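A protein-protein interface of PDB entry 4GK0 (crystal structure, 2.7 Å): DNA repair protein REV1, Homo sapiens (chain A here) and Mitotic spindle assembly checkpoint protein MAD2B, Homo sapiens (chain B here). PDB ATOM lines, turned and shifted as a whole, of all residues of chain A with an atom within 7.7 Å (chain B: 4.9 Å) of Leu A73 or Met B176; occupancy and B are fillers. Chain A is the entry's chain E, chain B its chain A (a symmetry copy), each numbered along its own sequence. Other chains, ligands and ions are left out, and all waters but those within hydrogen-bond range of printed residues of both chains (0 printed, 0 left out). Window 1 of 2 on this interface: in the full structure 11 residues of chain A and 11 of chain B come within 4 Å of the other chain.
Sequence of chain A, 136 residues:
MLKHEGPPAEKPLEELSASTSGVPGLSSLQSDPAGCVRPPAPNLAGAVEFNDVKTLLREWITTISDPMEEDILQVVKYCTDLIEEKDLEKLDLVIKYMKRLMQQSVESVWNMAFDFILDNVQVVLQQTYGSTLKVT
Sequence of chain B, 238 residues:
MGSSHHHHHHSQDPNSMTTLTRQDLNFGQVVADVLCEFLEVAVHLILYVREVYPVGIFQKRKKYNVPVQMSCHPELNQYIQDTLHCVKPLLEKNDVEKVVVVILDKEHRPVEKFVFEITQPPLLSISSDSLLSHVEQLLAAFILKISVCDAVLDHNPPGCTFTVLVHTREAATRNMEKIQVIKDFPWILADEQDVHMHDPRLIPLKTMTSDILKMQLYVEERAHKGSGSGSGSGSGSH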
ATOM      1  N   LEU A  44      27.281  15.987  24.073  1.00  0.00           N
ATOM      2  CA  LEU A  44      27.179  14.709  24.768  1.00  0.00           C
ATOM      3  C   LEU A  44      27.089  14.908  26.277  1.00  0.00           C
ATOM      4  O   LEU A  44      28.060  15.308  26.919  1.00  0.00           O
ATOM      5  CB  LEU A  44      28.373  13.816  24.425  1.00  0.00           C
ATOM      6  CG  LEU A  44      28.129  12.306  24.486  1.00  0.00           C
ATOM      7  CD1 LEU A  44      26.736  11.966  23.976  1.00  0.00           C
ATOM      8  CD2 LEU A  44      29.190  11.558  23.694  1.00  0.00           C
ATOM      9  N   TRP A  60      34.704   6.400  28.859  1.00  0.00           N
ATOM     10  CA  TRP A  60      33.524   5.553  28.797  1.00  0.00           C
ATOM     11  C   TRP A  60      33.809   4.226  28.124  1.00  0.00           C
ATOM     12  O   TRP A  60      33.389   3.198  28.601  1.00  0.00           O
ATOM     13  CB  TRP A  60      32.394   6.295  28.097  1.00  0.00           C
ATOM     14  CG  TRP A  60      31.158   5.479  27.836  1.00  0.00           C
ATOM     15  CD1 TRP A  60      30.415   4.822  28.754  1.00  0.00           C
ATOM     16  CD2 TRP A  60      30.500   5.286  26.577  1.00  0.00           C
ATOM     17  NE1 TRP A  60      29.337   4.212  28.156  1.00  0.00           N
ATOM     18  CE2 TRP A  60      29.367   4.471  26.817  1.00  0.00           C
ATOM     19  CE3 TRP A  60      30.745   5.729  25.278  1.00  0.00           C
ATOM     20  CZ2 TRP A  60      28.485   4.080  25.802  1.00  0.00           C
ATOM     21  CZ3 TRP A  60      29.880   5.327  24.264  1.00  0.00           C
ATOM     22  CH2 TRP A  60      28.761   4.511  24.532  1.00  0.00           C
ATOM     23  N   MET A  68      25.384   0.505  28.830  1.00  0.00           N
ATOM     24  CA  MET A  68      23.968   0.802  28.714  1.00  0.00           C
ATOM     25  C   MET A  68      23.583   1.294  27.318  1.00  0.00           C
ATOM     26  O   MET A  68      24.033   2.343  26.864  1.00  0.00           O
ATOM     27  CB  MET A  68      23.596   1.892  29.720  1.00  0.00           C
ATOM     28  CG  MET A  68      23.916   1.504  31.146  1.00  0.00           C
ATOM     29  SD  MET A  68      23.067   2.526  32.364  1.00  0.00           S
ATOM     30  CE  MET A  68      23.616   4.191  31.943  1.00  0.00           C
ATOM     31  N   GLU A  69      22.744   0.508  26.656  1.00  0.00           N
ATOM     32  CA  GLU A  69      22.013   0.919  25.454  1.00  0.00           C
ATOM     33  C   GLU A  69      21.541   2.378  25.486  1.00  0.00           C
ATOM     34  O   GLU A  69      21.746   3.126  24.539  1.00  0.00           O
ATOM     35  CB  GLU A  69      20.807   0.010  25.284  1.00  0.00           C
ATOM     36  CG  GLU A  69      21.188  -1.440  25.050  1.00  0.00           C
ATOM     37  CD  GLU A  69      20.011  -2.266  24.596  1.00  0.00           C
ATOM     38  OE1 GLU A  69      18.876  -1.827  24.808  1.00  0.00           O
ATOM     39  OE2 GLU A  69      20.209  -3.344  24.026  1.00  0.00           O
ATOM     40  N   GLU A  70      20.930   2.791  26.586  1.00  0.00           N
ATOM     41  CA  GLU A  70      20.505   4.173  26.723  1.00  0.00           C
ATOM     42  C   GLU A  70      21.639   5.150  26.406  1.00  0.00           C
ATOM     43  O   GLU A  70      21.384   6.248  25.908  1.00  0.00           O
ATOM     44  CB  GLU A  70      19.931   4.436  28.113  1.00  0.00           C
ATOM     45  CG  GLU A  70      19.838   5.917  28.478  1.00  0.00           C
ATOM     46  CD  GLU A  70      18.464   6.356  28.997  1.00  0.00           C
ATOM     47  OE1 GLU A  70      17.907   5.745  29.964  1.00  0.00           O
ATOM     48  OE2 GLU A  70      17.941   7.348  28.425  1.00  0.00           O
ATOM     49  N   ASP A  71      22.880   4.754  26.684  1.00  0.00           N
ATOM     50  CA  ASP A  71      24.041   5.606  26.413  1.00  0.00           C
ATOM     51  C   ASP A  71      24.405   5.546  24.927  1.00  0.00           C
ATOM     52  O   ASP A  71      24.644   6.560  24.288  1.00  0.00           O
ATOM     53  CB  ASP A  71      25.262   5.158  27.231  1.00  0.00           C
ATOM     54  CG  ASP A  71      25.204   5.566  28.679  1.00  0.00           C
ATOM     55  OD1 ASP A  71      24.731   6.655  29.019  1.00  0.00           O
ATOM     56  OD2 ASP A  71      25.694   4.773  29.511  1.00  0.00           O
ATOM     57  N   ILE A  72      24.487   4.342  24.400  1.00  0.00           N
ATOM     58  CA  ILE A  72      24.748   4.145  22.990  1.00  0.00           C
ATOM     59  C   ILE A  72      23.838   5.068  22.160  1.00  0.00           C
ATOM     60  O   ILE A  72      24.317   5.901  21.386  1.00  0.00           O
ATOM     61  CB  ILE A  72      24.542   2.673  22.595  1.00  0.00           C
ATOM     62  CG1 ILE A  72      25.400   1.775  23.511  1.00  0.00           C
ATOM     63  CG2 ILE A  72      24.797   2.478  21.104  1.00  0.00           C
ATOM     64  CD1 ILE A  72      25.637   0.370  23.029  1.00  0.00           C
ATOM     65  N   LEU A  73      22.532   4.960  22.408  1.00  0.00           N
ATOM     66  CA  LEU A  73      21.506   5.829  21.805  1.00  0.00           C
ATOM     67  C   LEU A  73      21.760   7.333  21.903  1.00  0.00           C
ATOM     68  O   LEU A  73      21.574   8.038  20.923  1.00  0.00           O
ATOM     69  CB  LEU A  73      20.128   5.474  22.345  1.00  0.00           C
ATOM     70  CG  LEU A  73      19.642   4.058  22.043  1.00  0.00           C
ATOM     71  CD1 LEU A  73      18.423   3.779  22.878  1.00  0.00           C
ATOM     72  CD2 LEU A  73      19.294   3.838  20.602  1.00  0.00           C
ATOM     73  N   GLN A  74      22.232   7.811  23.051  1.00  0.00           N
ATOM     74  CA  GLN A  74      22.686   9.214  23.183  1.00  0.00           C
ATOM     75  C   GLN A  74      23.848   9.541  22.250  1.00  0.00           C
ATOM     76  O   GLN A  74      23.997  10.657  21.803  1.00  0.00           O
ATOM     77  CB  GLN A  74      23.191   9.530  24.596  1.00  0.00           C
ATOM     78  CG  GLN A  74      22.195   9.575  25.748  1.00  0.00           C
ATOM     79  CD  GLN A  74      20.794  10.103  25.404  1.00  0.00           C
ATOM     80  OE1 GLN A  74      20.599  11.046  24.625  1.00  0.00           O
ATOM     81  NE2 GLN A  74      19.796   9.495  26.032  1.00  0.00           N
ATOM     82  N   VAL A  75      24.698   8.567  21.987  1.00  0.00           N
ATOM     83  CA  VAL A  75      25.812   8.808  21.096  1.00  0.00           C
ATOM     84  C   VAL A  75      25.261   8.991  19.691  1.00  0.00           C
ATOM     85  O   VAL A  75      25.643   9.894  18.976  1.00  0.00           O
ATOM     86  CB  VAL A  75      26.846   7.641  21.086  1.00  0.00           C
ATOM     87  CG1 VAL A  75      27.797   7.822  19.925  1.00  0.00           C
ATOM     88  CG2 VAL A  75      27.603   7.527  22.403  1.00  0.00           C
ATOM     89  N   VAL A  76      24.389   8.088  19.283  1.00  0.00           N
ATOM     90  CA  VAL A  76      23.721   8.204  17.997  1.00  0.00           C
ATOM     91  C   VAL A  76      23.054   9.558  17.920  1.00  0.00           C
ATOM     92  O   VAL A  76      23.162  10.250  16.917  1.00  0.00           O
ATOM     93  CB  VAL A  76      22.637   7.115  17.825  1.00  0.00           C
ATOM     94  CG1 VAL A  76      21.816   7.357  16.572  1.00  0.00           C
ATOM     95  CG2 VAL A  76      23.260   5.722  17.810  1.00  0.00           C
ATOM     96  N   LYS A  77      22.338   9.929  18.973  1.00  0.00           N
ATOM     97  CA  LYS A  77      21.609  11.164  18.882  1.00  0.00           C
ATOM     98  C   LYS A  77      22.564  12.326  18.710  1.00  0.00           C
ATOM     99  O   LYS A  77      22.353  13.219  17.881  1.00  0.00           O
ATOM    100  CB  LYS A  77      20.739  11.395  20.087  1.00  0.00           C
ATOM    101  CG  LYS A  77      19.865  12.619  19.931  1.00  0.00           C
ATOM    102  CD  LYS A  77      19.075  12.769  21.214  1.00  0.00           C
ATOM    103  CE  LYS A  77      18.489  14.170  21.369  1.00  0.00           C
ATOM    104  NZ  LYS A  77      18.163  14.422  22.811  1.00  0.00           N
ATOM    105  N   TYR A  78      23.639  12.281  19.481  1.00  0.00           N
ATOM    106  CA  TYR A  78      24.627  13.338  19.465  1.00  0.00           C
ATOM    107  C   TYR A  78      25.185  13.505  18.049  1.00  0.00           C
ATOM    108  O   TYR A  78      25.297  14.604  17.496  1.00  0.00           O
ATOM    109  CB  TYR A  78      25.720  13.026  20.489  1.00  0.00           C
ATOM    110  CG  TYR A  78      26.910  13.885  20.294  1.00  0.00           C
ATOM    111  CD1 TYR A  78      26.867  15.231  20.647  1.00  0.00           C
ATOM    112  CD2 TYR A  78      28.057  13.385  19.689  1.00  0.00           C
ATOM    113  CE1 TYR A  78      27.954  16.055  20.443  1.00  0.00           C
ATOM    114  CE2 TYR A  78      29.141  14.219  19.451  1.00  0.00           C
ATOM    115  CZ  TYR A  78      29.079  15.547  19.844  1.00  0.00           C
ATOM    116  OH  TYR A  78      30.116  16.387  19.633  1.00  0.00           O
ATOM    117  N   CYS A  79      25.481  12.384  17.429  1.00  0.00           N
ATOM    118  CA  CYS A  79      25.917  12.408  16.057  1.00  0.00           C
ATOM    119  C   CYS A  79      24.880  12.942  15.058  1.00  0.00           C
ATOM    120  O   CYS A  79      25.257  13.556  14.036  1.00  0.00           O
ATOM    121  CB  CYS A  79      26.383  11.006  15.653  1.00  0.00           C
ATOM    122  SG  CYS A  79      27.823  10.446  16.616  1.00  0.00           S
ATOM    123  N   THR A  80      23.587  12.731  15.295  1.00  0.00           N
ATOM    124  CA  THR A  80      22.650  13.144  14.266  1.00  0.00           C
ATOM    125  C   THR A  80      22.383  14.602  14.457  1.00  0.00           C
ATOM    126  O   THR A  80      22.203  15.330  13.483  1.00  0.00           O
ATOM    127  CB  THR A  80      21.387  12.291  14.143  1.00  0.00           C
ATOM    128  OG1 THR A  80      20.738  12.168  15.408  1.00  0.00           O
ATOM    129  CG2 THR A  80      21.731  10.908  13.658  1.00  0.00           C
ATOM    130  N   PHE A 116      26.430  -0.209  15.154  1.00  0.00           N
ATOM    131  CA  PHE A 116      25.075   0.305  15.307  1.00  0.00           C
ATOM    132  C   PHE A 116      25.061   1.824  15.114  1.00  0.00           C
ATOM    133  O   PHE A 116      24.269   2.343  14.351  1.00  0.00           O
ATOM    134  CB  PHE A 116      24.512  -0.130  16.658  1.00  0.00           C
ATOM    135  CG  PHE A 116      23.259   0.584  17.087  1.00  0.00           C
ATOM    136  CD1 PHE A 116      22.006   0.150  16.664  1.00  0.00           C
ATOM    137  CD2 PHE A 116      23.334   1.662  17.995  1.00  0.00           C
ATOM    138  CE1 PHE A 116      20.841   0.799  17.087  1.00  0.00           C
ATOM    139  CE2 PHE A 116      22.173   2.310  18.427  1.00  0.00           C
ATOM    140  CZ  PHE A 116      20.912   1.881  17.962  1.00  0.00           C
ATOM    141  N   ILE A 117      25.969   2.511  15.788  1.00  0.00           N
ATOM    142  CA  ILE A 117      26.040   3.952  15.747  1.00  0.00           C
ATOM    143  C   ILE A 117      26.262   4.415  14.314  1.00  0.00           C
ATOM    144  O   ILE A 117      25.650   5.395  13.891  1.00  0.00           O
ATOM    145  CB  ILE A 117      27.142   4.468  16.690  1.00  0.00           C
ATOM    146  CG1 ILE A 117      26.775   4.190  18.160  1.00  0.00           C
ATOM    147  CG2 ILE A 117      27.353   5.951  16.485  1.00  0.00           C
ATOM    148  CD1 ILE A 117      27.863   4.408  19.235  1.00  0.00           C
ATOM    149  N   ASN A 120      23.284   4.020  11.932  1.00  0.00           N
ATOM    150  CA  ASN A 120      22.258   5.028  12.167  1.00  0.00           C
ATOM    151  C   ASN A 120      22.697   6.440  11.772  1.00  0.00           C
ATOM    152  O   ASN A 120      21.878   7.303  11.581  1.00  0.00           O
ATOM    153  CB  ASN A 120      21.768   4.987  13.618  1.00  0.00           C
ATOM    154  CG  ASN A 120      20.868   3.814  13.873  1.00  0.00           C
ATOM    155  OD1 ASN A 120      19.756   3.807  13.413  1.00  0.00           O
ATOM    156  ND2 ASN A 120      21.350   2.803  14.582  1.00  0.00           N
ATOM    157  N   VAL A 121      23.993   6.668  11.654  1.00  0.00           N
ATOM    158  CA  VAL A 121      24.494   7.932  11.202  1.00  0.00           C
ATOM    159  C   VAL A 121      24.467   7.925   9.680  1.00  0.00           C
ATOM    160  O   VAL A 121      24.118   8.906   9.049  1.00  0.00           O
ATOM    161  CB  VAL A 121      25.915   8.154  11.759  1.00  0.00           C
ATOM    162  CG1 VAL A 121      26.683   9.248  11.011  1.00  0.00           C
ATOM    163  CG2 VAL A 121      25.820   8.493  13.228  1.00  0.00           C
ATOM    164  N   VAL A 123      22.336   6.400   7.520  1.00  0.00           N
ATOM    165  CA  VAL A 123      21.060   6.564   6.829  1.00  0.00           C
ATOM    166  C   VAL A 123      20.663   8.007   6.922  1.00  0.00           C
ATOM    167  O   VAL A 123      20.043   8.532   6.013  1.00  0.00           O
ATOM    168  CB  VAL A 123      19.916   5.661   7.346  1.00  0.00           C
ATOM    169  CG1 VAL A 123      20.235   4.220   7.119  1.00  0.00           C
ATOM    170  CG2 VAL A 123      19.679   5.844   8.823  1.00  0.00           C
ATOM    171  N   ALA B 171      14.347   2.338  26.497  1.00  0.00           N
ATOM    172  CA  ALA B 171      15.369   2.945  25.643  1.00  0.00           C
ATOM    173  C   ALA B 171      16.358   1.835  25.213  1.00  0.00           C
ATOM    174  O   ALA B 171      17.354   1.542  25.897  1.00  0.00           O
ATOM    175  CB  ALA B 171      16.098   4.069  26.356  1.00  0.00           C
ATOM    176  N   ALA B 172      16.065   1.233  24.069  1.00  0.00           N
ATOM    177  CA  ALA B 172      16.664   0.011  23.658  1.00  0.00           C
ATOM    178  C   ALA B 172      17.113   0.127  22.229  1.00  0.00           C
ATOM    179  O   ALA B 172      16.412   0.553  21.335  1.00  0.00           O
ATOM    180  CB  ALA B 172      15.690  -1.139  23.796  1.00  0.00           C
ATOM    181  N   THR B 173      18.336  -0.301  22.034  1.00  0.00           N
ATOM    182  CA  THR B 173      18.918  -0.438  20.735  1.00  0.00           C
ATOM    183  C   THR B 173      17.984  -1.032  19.691  1.00  0.00           C
ATOM    184  O   THR B 173      17.886  -0.524  18.590  1.00  0.00           O
ATOM    185  CB  THR B 173      20.223  -1.223  20.917  1.00  0.00           C
ATOM    186  OG1 THR B 173      21.301  -0.416  20.441  1.00  0.00           O
ATOM    187  CG2 THR B 173      20.197  -2.635  20.262  1.00  0.00           C
ATOM    188  N   ARG B 174      17.253  -2.070  20.056  1.00  0.00           N
ATOM    189  CA  ARG B 174      16.538  -2.888  19.084  1.00  0.00           C
ATOM    190  C   ARG B 174      15.371  -2.154  18.443  1.00  0.00           C
ATOM    191  O   ARG B 174      14.914  -2.546  17.356  1.00  0.00           O
ATOM    192  CB  ARG B 174      16.038  -4.189  19.739  1.00  0.00           C
ATOM    193  CG  ARG B 174      14.668  -4.094  20.407  1.00  0.00           C
ATOM    194  CD  ARG B 174      14.396  -5.131  21.509  1.00  0.00           C
ATOM    195  NE  ARG B 174      14.403  -4.512  22.856  1.00  0.00           N
ATOM    196  CZ  ARG B 174      13.324  -4.270  23.612  1.00  0.00           C
ATOM    197  NH1 ARG B 174      12.118  -4.605  23.198  1.00  0.00           N
ATOM    198  NH2 ARG B 174      13.437  -3.683  24.802  1.00  0.00           N
ATOM    199  N   ASN B 175      14.863  -1.136  19.149  1.00  0.00           N
ATOM    200  CA  ASN B 175      13.777  -0.309  18.633  1.00  0.00           C
ATOM    201  C   ASN B 175      14.285   0.376  17.366  1.00  0.00           C
ATOM    202  O   ASN B 175      13.635   0.306  16.321  1.00  0.00           O
ATOM    203  CB  ASN B 175      13.256   0.680  19.676  1.00  0.00           C
ATOM    204  CG  ASN B 175      12.662  -0.004  20.900  1.00  0.00           C
ATOM    205  OD1 ASN B 175      12.083  -1.062  20.788  1.00  0.00           O
ATOM    206  ND2 ASN B 175      12.801   0.615  22.083  1.00  0.00           N
ATOM    207  N   MET B 176      15.491   0.955  17.436  1.00  0.00           N
ATOM    208  CA  MET B 176      16.129   1.532  16.249  1.00  0.00           C
ATOM    209  C   MET B 176      16.476   0.558  15.148  1.00  0.00           C
ATOM    210  O   MET B 176      16.232   0.841  14.015  1.00  0.00           O
ATOM    211  CB  MET B 176      17.357   2.317  16.603  1.00  0.00           C
ATOM    212  CG  MET B 176      17.051   3.726  17.046  1.00  0.00           C
ATOM    213  SD  MET B 176      18.209   4.892  16.285  1.00  0.00           S
ATOM    214  CE  MET B 176      18.275   6.082  17.618  1.00  0.00           C
ATOM    215  N   GLU B 177      17.071  -0.577  15.454  1.00  0.00           N
ATOM    216  CA  GLU B 177      17.239  -1.605  14.426  1.00  0.00           C
ATOM    217  C   GLU B 177      15.893  -1.880  13.750  1.00  0.00           C
ATOM    218  O   GLU B 177      15.787  -1.817  12.544  1.00  0.00           O
ATOM    219  CB  GLU B 177      17.755  -2.928  15.028  1.00  0.00           C
ATOM    220  CG  GLU B 177      19.270  -3.164  14.972  1.00  0.00           C
ATOM    221  CD  GLU B 177      19.814  -3.874  16.217  1.00  0.00           C
ATOM    222  OE1 GLU B 177      19.243  -4.904  16.652  1.00  0.00           O
ATOM    223  OE2 GLU B 177      20.809  -3.384  16.785  1.00  0.00           O
ATOM    224  N   LYS B 178      14.877  -2.209  14.541  1.00  0.00           N
ATOM    225  CA  LYS B 178      13.577  -2.581  13.992  1.00  0.00           C
ATOM    226  C   LYS B 178      12.879  -1.461  13.201  1.00  0.00           C
ATOM    227  O   LYS B 178      12.239  -1.722  12.198  1.00  0.00           O
ATOM    228  CB  LYS B 178      12.661  -3.134  15.092  1.00  0.00           C
ATOM    229  CG  LYS B 178      12.972  -4.569  15.483  1.00  0.00           C
ATOM    230  CD  LYS B 178      12.153  -5.080  16.659  1.00  0.00           C
ATOM    231  CE  LYS B 178      12.535  -6.541  16.903  1.00  0.00           C
ATOM    232  NZ  LYS B 178      12.608  -6.999  18.329  1.00  0.00           N
ATOM    233  N   ILE B 179      13.051  -0.219  13.624  1.00  0.00           N
ATOM    234  CA  ILE B 179      12.400   0.903  12.960  1.00  0.00           C
ATOM    235  C   ILE B 179      13.062   1.304  11.648  1.00  0.00           C
ATOM    236  O   ILE B 179      12.459   1.893  10.780  1.00  0.00           O
ATOM    237  CB  ILE B 179      12.307   2.130  13.889  1.00  0.00           C
ATOM    238  CG1 ILE B 179      11.063   2.951  13.522  1.00  0.00           C
ATOM    239  CG2 ILE B 179      13.594   2.928  13.857  1.00  0.00           C
ATOM    240  CD1 ILE B 179      10.444   3.705  14.693  1.00  0.00           C
ATOM    241  N   GLN B 180      14.319   0.944  11.513  1.00  0.00           N
ATOM    242  CA  GLN B 180      15.185   1.538  10.522  1.00  0.00           C
ATOM    243  C   GLN B 180      15.146   0.683   9.266  1.00  0.00           C
ATOM    244  O   GLN B 180      16.154   0.341   8.716  1.00  0.00           O
ATOM    245  CB  GLN B 180      16.564   1.682  11.152  1.00  0.00           C
ATOM    246  CG  GLN B 180      17.350   2.870  10.733  1.00  0.00           C
ATOM    247  CD  GLN B 180      16.732   4.200  11.133  1.00  0.00           C
ATOM    248  OE1 GLN B 180      17.113   4.812  12.128  1.00  0.00           O
ATOM    249  NE2 GLN B 180      15.803   4.668  10.323  1.00  0.00           N
ATOM    250  N   LEU B 189      16.270  10.025  17.024  1.00  0.00           N
ATOM    251  CA  LEU B 189      15.750  10.333  18.358  1.00  0.00           C
ATOM    252  C   LEU B 189      15.314  11.781  18.376  1.00  0.00           C
ATOM    253  O   LEU B 189      15.942  12.630  17.764  1.00  0.00           O
ATOM    254  CB  LEU B 189      16.772  10.056  19.469  1.00  0.00           C
ATOM    255  CG  LEU B 189      17.240   8.582  19.467  1.00  0.00           C
ATOM    256  CD1 LEU B 189      18.615   8.441  20.057  1.00  0.00           C
ATOM    257  CD2 LEU B 189      16.294   7.585  20.131  1.00  0.00           C
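The backbone NH (N) of Thr B173 sits at hydrogen-bond distance from the side-chain carboxylate (OE1) of Glu A69 (3.2 Å).
OE1 of Gln B180 lies close to OD1 of Asn A120.
The side-chain sulfur (SD) of Met B176 sits close to the side-chain amide oxygen (OD1) of Asn A120 (3.4 Å).
O of Lys A77 sits at hydrogen-bond distance from OG1 of Thr A80, at 3.1 Å.
OG1 of Thr A80 sits at hydrogen-bond distance from O of Val A76 (3.4 Å).
The side-chain amide nitrogen of Asn A120 sits at hydrogen-bond distance from the backbone carbonyl oxygen of Phe A116, 3.0 Å away.
O of Ala B171 touches CB of Glu A69, at 3.8 Å.
CA of Ala B172 touches OE1 of Glu A69, at 3.1 Å.
Glu A70 touches Ala B171 (N to O, 3.8 Å).
CD1 of Leu A73 touches C of Ala B171, 3.7 Å away.
Leu B189 touches Leu A73 (CD1 to O, 3.1 Å).
Met B176 touches Val A76 (CE to CG1, 3.9 Å).
Leu B189 touches Lys A77 (CD1 to CB, 3.6 Å).
CZ of Phe A116 touches OG1 of Thr B173, at 3.4 Å.
Phe A116 touches Met B176 (CZ to CB, 3.8 Å).
Glu B177 touches Phe A116.
Of chain B, only Ala B171 (3.7 Å), Ala B172 (3.7 Å), Met B176 (3.9 Å) and Leu B189 (3.1 Å) come within 4 Å of Leu A73.
Met B176 touches just these residues of chain A: Leu A73, Val A76, Phe A116 and Asn A120.
Printed residues of chain A within 4 Å of Gln B180: Asn A120.
Of the printed residues of chain B, Glu A69 touches Ala B171, Ala B172 and Thr B173.
The nearest residue of chain A that does not touch Met B176 is Lys A77 (5.8 Å).
The nearest printed residue of chain A that does not touch Gln B180 is Val A123 (4.1 Å).
Of the 20 printed residues of chain A, 7 touch a printed residue of chain B.
Of the 11 printed residues of chain B, 7 touch a printed residue of chain A.
Hydrophobic or aromatic side chains of chain B within 4 Å of the printed part of chain A: Ala B172, Met B176 and Leu B189.
Among the printed residues, 15 pairs touch across the chains.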
